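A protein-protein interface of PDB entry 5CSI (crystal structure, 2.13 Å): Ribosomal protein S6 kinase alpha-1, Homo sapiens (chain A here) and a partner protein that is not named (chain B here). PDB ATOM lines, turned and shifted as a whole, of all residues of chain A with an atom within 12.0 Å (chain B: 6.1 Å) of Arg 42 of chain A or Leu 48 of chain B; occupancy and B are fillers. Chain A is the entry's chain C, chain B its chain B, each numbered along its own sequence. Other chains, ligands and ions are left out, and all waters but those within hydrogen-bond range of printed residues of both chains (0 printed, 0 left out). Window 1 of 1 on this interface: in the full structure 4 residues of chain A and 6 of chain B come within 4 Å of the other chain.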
ATOM      1  N   ARG A  39     -21.869  -1.464  26.082  1.00  0.00           N
ATOM      2  CA  ARG A  39     -21.017  -1.103  24.956  1.00  0.00           C
ATOM      3  C   ARG A  39     -20.360  -2.328  24.326  1.00  0.00           C
ATOM      4  O   ARG A  39     -19.179  -2.292  23.981  1.00  0.00           O
ATOM      5  CB  ARG A  39     -19.943  -0.107  25.394  1.00  0.00           C
ATOM      6  N   ARG A  40     -21.128  -3.407  24.180  1.00  0.00           N
ATOM      7  CA  ARG A  40     -20.645  -4.627  23.529  1.00  0.00           C
ATOM      8  C   ARG A  40     -21.800  -5.509  23.044  1.00  0.00           C
ATOM      9  O   ARG A  40     -22.671  -5.896  23.823  1.00  0.00           O
ATOM     10  CB  ARG A  40     -19.744  -5.420  24.480  1.00  0.00           C
ATOM     11  N   VAL A  41     -21.794  -5.825  21.751  1.00  0.00           N
ATOM     12  CA  VAL A  41     -22.861  -6.609  21.133  1.00  0.00           C
ATOM     13  C   VAL A  41     -22.661  -8.102  21.393  1.00  0.00           C
ATOM     14  O   VAL A  41     -21.534  -8.593  21.387  1.00  0.00           O
ATOM     15  CB  VAL A  41     -22.930  -6.352  19.600  1.00  0.00           C
ATOM     16  CG1 VAL A  41     -24.077  -7.116  18.960  1.00  0.00           C
ATOM     17  CG2 VAL A  41     -23.075  -4.867  19.313  1.00  0.00           C
ATOM     18  N   ARG A  42     -23.754  -8.823  21.631  1.00  0.00           N
ATOM     19  CA  ARG A  42     -23.683 -10.272  21.759  1.00  0.00           C
ATOM     20  C   ARG A  42     -23.377 -10.908  20.406  1.00  0.00           C
ATOM     21  O   ARG A  42     -23.130 -10.211  19.422  1.00  0.00           O
ATOM     22  CB  ARG A  42     -24.987 -10.834  22.325  1.00  0.00           C
ATOM     23  CG  ARG A  42     -25.303 -10.357  23.729  1.00  0.00           C
ATOM     24  CD  ARG A  42     -26.082 -11.410  24.506  1.00  0.00           C
ATOM     25  NE  ARG A  42     -25.504 -11.648  25.828  1.00  0.00           N
ATOM     26  CZ  ARG A  42     -25.967 -11.129  26.963  1.00  0.00           C
ATOM     27  NH1 ARG A  42     -27.034 -10.340  26.951  1.00  0.00           N
ATOM     28  NH2 ARG A  42     -25.367 -11.404  28.116  1.00  0.00           N
ATOM     29  N   LYS A  43     -23.390 -12.234  20.356  1.00  0.00           N
ATOM     30  CA  LYS A  43     -23.143 -12.934  19.104  1.00  0.00           C
ATOM     31  C   LYS A  43     -24.377 -12.880  18.202  1.00  0.00           C
ATOM     32  O   LYS A  43     -24.256 -12.635  17.002  1.00  0.00           O
ATOM     33  CB  LYS A  43     -22.736 -14.384  19.372  1.00  0.00           C
ATOM     34  N   LEU A  44     -25.552 -13.073  18.807  1.00  0.00           N
ATOM     35  CA  LEU A  44     -26.856 -13.187  18.123  1.00  0.00           C
ATOM     36  C   LEU A  44     -26.865 -14.070  16.868  1.00  0.00           C
ATOM     37  O   LEU A  44     -26.345 -13.683  15.820  1.00  0.00           O
ATOM     38  CB  LEU A  44     -27.427 -11.802  17.758  1.00  0.00           C
ATOM     39  CG  LEU A  44     -26.600 -10.554  17.436  1.00  0.00           C
ATOM     40  CD1 LEU A  44     -27.385  -9.598  16.558  1.00  0.00           C
ATOM     41  CD2 LEU A  44     -26.219  -9.869  18.723  1.00  0.00           C
ATOM     42  N   PRO A  45     -27.490 -15.256  16.970  1.00  0.00           N
ATOM     43  CA  PRO A  45     -27.636 -16.176  15.836  1.00  0.00           C
ATOM     44  C   PRO A  45     -28.773 -15.774  14.899  1.00  0.00           C
ATOM     45  O   PRO A  45     -29.767 -16.498  14.812  1.00  0.00           O
ATOM     46  CB  PRO A  45     -27.938 -17.513  16.515  1.00  0.00           C
ATOM     47  CG  PRO A  45     -28.661 -17.126  17.760  1.00  0.00           C
ATOM     48  CD  PRO A  45     -28.067 -15.812  18.208  1.00  0.00           C
ATOM     49  N   ILE B  40     -30.915  -1.825  30.003  1.00  0.00           N
ATOM     50  CA  ILE B  40     -30.077  -2.608  29.109  1.00  0.00           C
ATOM     51  C   ILE B  40     -30.125  -4.094  29.463  1.00  0.00           C
ATOM     52  O   ILE B  40     -30.245  -4.945  28.577  1.00  0.00           O
ATOM     53  CB  ILE B  40     -28.632  -2.109  29.146  1.00  0.00           C
ATOM     54  CG1 ILE B  40     -28.539  -0.725  28.507  1.00  0.00           C
ATOM     55  CG2 ILE B  40     -27.689  -3.092  28.455  1.00  0.00           C
ATOM     56  CD1 ILE B  40     -27.180  -0.093  28.666  1.00  0.00           C
ATOM     57  N   LEU B  44     -32.598  -5.383  26.635  1.00  0.00           N
ATOM     58  CA  LEU B  44     -31.669  -5.524  25.530  1.00  0.00           C
ATOM     59  C   LEU B  44     -30.782  -6.747  25.680  1.00  0.00           C
ATOM     60  O   LEU B  44     -29.668  -6.786  25.160  1.00  0.00           O
ATOM     61  CB  LEU B  44     -30.809  -4.264  25.407  1.00  0.00           C
ATOM     62  CG  LEU B  44     -31.492  -3.019  24.832  1.00  0.00           C
ATOM     63  CD1 LEU B  44     -30.519  -1.870  24.858  1.00  0.00           C
ATOM     64  CD2 LEU B  44     -31.977  -3.271  23.393  1.00  0.00           C
ATOM     65  N   SER B  45     -31.291  -7.768  26.357  1.00  0.00           N
ATOM     66  CA  SER B  45     -30.465  -8.907  26.724  1.00  0.00           C
ATOM     67  C   SER B  45     -30.062  -9.748  25.509  1.00  0.00           C
ATOM     68  O   SER B  45     -29.128 -10.542  25.587  1.00  0.00           O
ATOM     69  CB  SER B  45     -31.194  -9.776  27.748  1.00  0.00           C
ATOM     70  OG  SER B  45     -32.357 -10.341  27.169  1.00  0.00           O
ATOM     71  N   HIS B  46     -30.749  -9.566  24.386  1.00  0.00           N
ATOM     72  CA  HIS B  46     -30.404 -10.322  23.182  1.00  0.00           C
ATOM     73  C   HIS B  46     -29.463  -9.563  22.239  1.00  0.00           C
ATOM     74  O   HIS B  46     -28.895 -10.153  21.325  1.00  0.00           O
ATOM     75  CB  HIS B  46     -31.670 -10.723  22.430  1.00  0.00           C
ATOM     76  CG  HIS B  46     -32.687 -11.401  23.290  1.00  0.00           C
ATOM     77  ND1 HIS B  46     -33.686 -10.713  23.941  1.00  0.00           N
ATOM     78  CD2 HIS B  46     -32.857 -12.707  23.605  1.00  0.00           C
ATOM     79  CE1 HIS B  46     -34.432 -11.567  24.620  1.00  0.00           C
ATOM     80  NE2 HIS B  46     -33.952 -12.782  24.434  1.00  0.00           N
ATOM     81  N   PHE B  47     -29.291  -8.265  22.462  1.00  0.00           N
ATOM     82  CA  PHE B  47     -28.431  -7.455  21.594  1.00  0.00           C
ATOM     83  C   PHE B  47     -27.138  -7.024  22.299  1.00  0.00           C
ATOM     84  O   PHE B  47     -26.075  -6.977  21.680  1.00  0.00           O
ATOM     85  CB  PHE B  47     -29.178  -6.209  21.093  1.00  0.00           C
ATOM     86  CG  PHE B  47     -30.364  -6.508  20.195  1.00  0.00           C
ATOM     87  CD1 PHE B  47     -30.532  -7.750  19.605  1.00  0.00           C
ATOM     88  CD2 PHE B  47     -31.311  -5.526  19.942  1.00  0.00           C
ATOM     89  CE1 PHE B  47     -31.629  -8.007  18.785  1.00  0.00           C
ATOM     90  CE2 PHE B  47     -32.405  -5.780  19.115  1.00  0.00           C
ATOM     91  CZ  PHE B  47     -32.566  -7.012  18.544  1.00  0.00           C
ATOM     92  N   LEU B  48     -27.234  -6.709  23.590  1.00  0.00           N
ATOM     93  CA  LEU B  48     -26.074  -6.284  24.367  1.00  0.00           C
ATOM     94  C   LEU B  48     -25.702  -7.263  25.476  1.00  0.00           C
ATOM     95  O   LEU B  48     -26.572  -7.826  26.136  1.00  0.00           O
ATOM     96  CB  LEU B  48     -26.328  -4.913  24.990  1.00  0.00           C
ATOM     97  CG  LEU B  48     -26.665  -3.789  24.018  1.00  0.00           C
ATOM     98  CD1 LEU B  48     -26.791  -2.472  24.773  1.00  0.00           C
ATOM     99  CD2 LEU B  48     -25.603  -3.711  22.946  1.00  0.00           C
ATOM    100  N   GLU B  49     -24.404  -7.443  25.687  1.00  0.00           N
ATOM    101  CA  GLU B  49     -23.930  -8.241  26.800  1.00  0.00           C
ATOM    102  C   GLU B  49     -24.379  -7.602  28.106  1.00  0.00           C
ATOM    103  O   GLU B  49     -24.450  -6.379  28.210  1.00  0.00           O
ATOM    104  CB  GLU B  49     -22.410  -8.389  26.754  1.00  0.00           C
ATOM    105  CG  GLU B  49     -21.962  -9.824  26.547  1.00  0.00           C
ATOM    106  CD  GLU B  49     -20.543  -9.929  26.041  1.00  0.00           C
ATOM    107  OE1 GLU B  49     -19.662  -9.245  26.600  1.00  0.00           O
ATOM    108  OE2 GLU B  49     -20.316 -10.694  25.079  1.00  0.00           O
ATOM    109  N   GLU B  50     -24.718  -8.436  29.086  1.00  0.00           N
ATOM    110  CA  GLU B  50     -25.176  -7.949  30.383  1.00  0.00           C
ATOM    111  C   GLU B  50     -24.170  -6.988  30.991  1.00  0.00           C
ATOM    112  O   GLU B  50     -22.968  -7.172  30.837  1.00  0.00           O
ATOM    113  CB  GLU B  50     -25.411  -9.117  31.338  1.00  0.00           C
ATOM    114  CG  GLU B  50     -25.935  -8.708  32.696  1.00  0.00           C
ATOM    115  CD  GLU B  50     -26.210  -9.900  33.584  1.00  0.00           C
ATOM    116  OE1 GLU B  50     -26.031 -11.041  33.114  1.00  0.00           O
ATOM    117  OE2 GLU B  50     -26.600  -9.698  34.748  1.00  0.00           O
ATOM    118  N   PHE B  80     -28.878   6.712  21.646  1.00  0.00           N
ATOM    119  CA  PHE B  80     -28.457   5.389  22.091  1.00  0.00           C
ATOM    120  C   PHE B  80     -29.120   4.311  21.231  1.00  0.00           C
ATOM    121  O   PHE B  80     -28.450   3.412  20.719  1.00  0.00           O
ATOM    122  CB  PHE B  80     -28.801   5.172  23.570  1.00  0.00           C
ATOM    123  CG  PHE B  80     -28.426   3.801  24.094  1.00  0.00           C
ATOM    124  CD1 PHE B  80     -27.104   3.377  24.084  1.00  0.00           C
ATOM    125  CD2 PHE B  80     -29.392   2.956  24.626  1.00  0.00           C
ATOM    126  CE1 PHE B  80     -26.748   2.127  24.572  1.00  0.00           C
ATOM    127  CE2 PHE B  80     -29.042   1.698  25.119  1.00  0.00           C
ATOM    128  CZ  PHE B  80     -27.718   1.286  25.089  1.00  0.00           C
ATOM    129  N   VAL B  84     -27.252   1.538  18.829  1.00  0.00           N
ATOM    130  CA  VAL B  84     -27.420   0.093  18.963  1.00  0.00           C
ATOM    131  C   VAL B  84     -28.043  -0.532  17.721  1.00  0.00           C
ATOM    132  O   VAL B  84     -27.531  -1.507  17.186  1.00  0.00           O
ATOM    133  CB  VAL B  84     -28.300  -0.269  20.172  1.00  0.00           C
ATOM    134  CG1 VAL B  84     -28.396  -1.789  20.318  1.00  0.00           C
ATOM    135  CG2 VAL B  84     -27.744   0.372  21.442  1.00  0.00           C
ATOM    136  N   PHE B  91     -25.365  -7.079  11.441  1.00  0.00           N
ATOM    137  CA  PHE B  91     -25.473  -8.528  11.613  1.00  0.00           C
ATOM    138  C   PHE B  91     -26.836  -9.029  11.136  1.00  0.00           C
ATOM    139  O   PHE B  91     -27.451  -9.873  11.789  1.00  0.00           O
ATOM    140  CB  PHE B  91     -25.269  -8.941  13.081  1.00  0.00           C
ATOM    141  CG  PHE B  91     -23.927  -8.556  13.675  1.00  0.00           C
ATOM    142  CD1 PHE B  91     -22.980  -7.846  12.946  1.00  0.00           C
ATOM    143  CD2 PHE B  91     -23.618  -8.921  14.978  1.00  0.00           C
ATOM    144  CE1 PHE B  91     -21.762  -7.500  13.509  1.00  0.00           C
ATOM    145  CE2 PHE B  91     -22.401  -8.582  15.543  1.00  0.00           C
ATOM    146  CZ  PHE B  91     -21.472  -7.872  14.808  1.00  0.00           C
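O of Arg 40 of chain A touches CA of Leu 48 of chain B, at 3.5 Å. CA of Val 41 of chain A touches O of Phe 47 of chain B (3.3 Å). CA of Glu 49 of chain B touches CZ of Arg 42 of chain A (3.5 Å). His 46 of chain B touches Leu 44 of chain A.
Of the 7 printed residues of chain A, 4 touch a printed residue of chain B. Hydrophobic or aromatic side chains of chain A within 4 Å of the printed part of chain B: Val 41 and Leu 44. Along chain A the printed residues that touch a printed residue of chain B span positions 40 to 44. Among the printed residues, 9 pairs touch across the chains.
Arg 42 of chain A touches five residues of chain B. No residue of chain A comes within 4 Å of Ile 40 of chain B. Ser 45 of chain B touches one residue of chain A. His 46 of chain B touches just one residue of chain A: Leu 44 (3.7 Å). Val 84 of chain B touches none of the printed residues of chain A. Of the printed residues of chain B, Val 41 of chain A touches Phe 47 (3.3 Å). Of the printed residues of chain B, Leu 44 of chain A touches His 46 (3.7 Å). Printed residues of chain B within 4 Å of Arg 40 of chain A: Leu 48 and Glu 49. Pro 45 of chain A touches none of the printed residues of chain B. The nearest residue of chain A that does not touch Leu 48 of chain B is Val 41 of chain A (4.4 Å).
NH1 of Arg 42 of chain A sits at hydrogen-bond distance from O of Leu 48 of chain B (2.7 Å). The guanidinium group (NH2) of Arg 42 of chain A sits close to the backbone NH (N) of Glu 50 of chain B. The backbone carbonyl oxygen (O) of Phe 47 of chain B sits at hydrogen-bond distance from the backbone NH (N) of Arg 42 of chain A, at 3.0 Å. N of Glu 49 of chain B sits at hydrogen-bond distance from O of Arg 40 of chain A, at 3.0 Å. The backbone carbonyl oxygen of Ser 45 of chain B lies within hydrogen-bond range of the guanidinium group of Arg 42 of chain A, at 2.5 Å.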
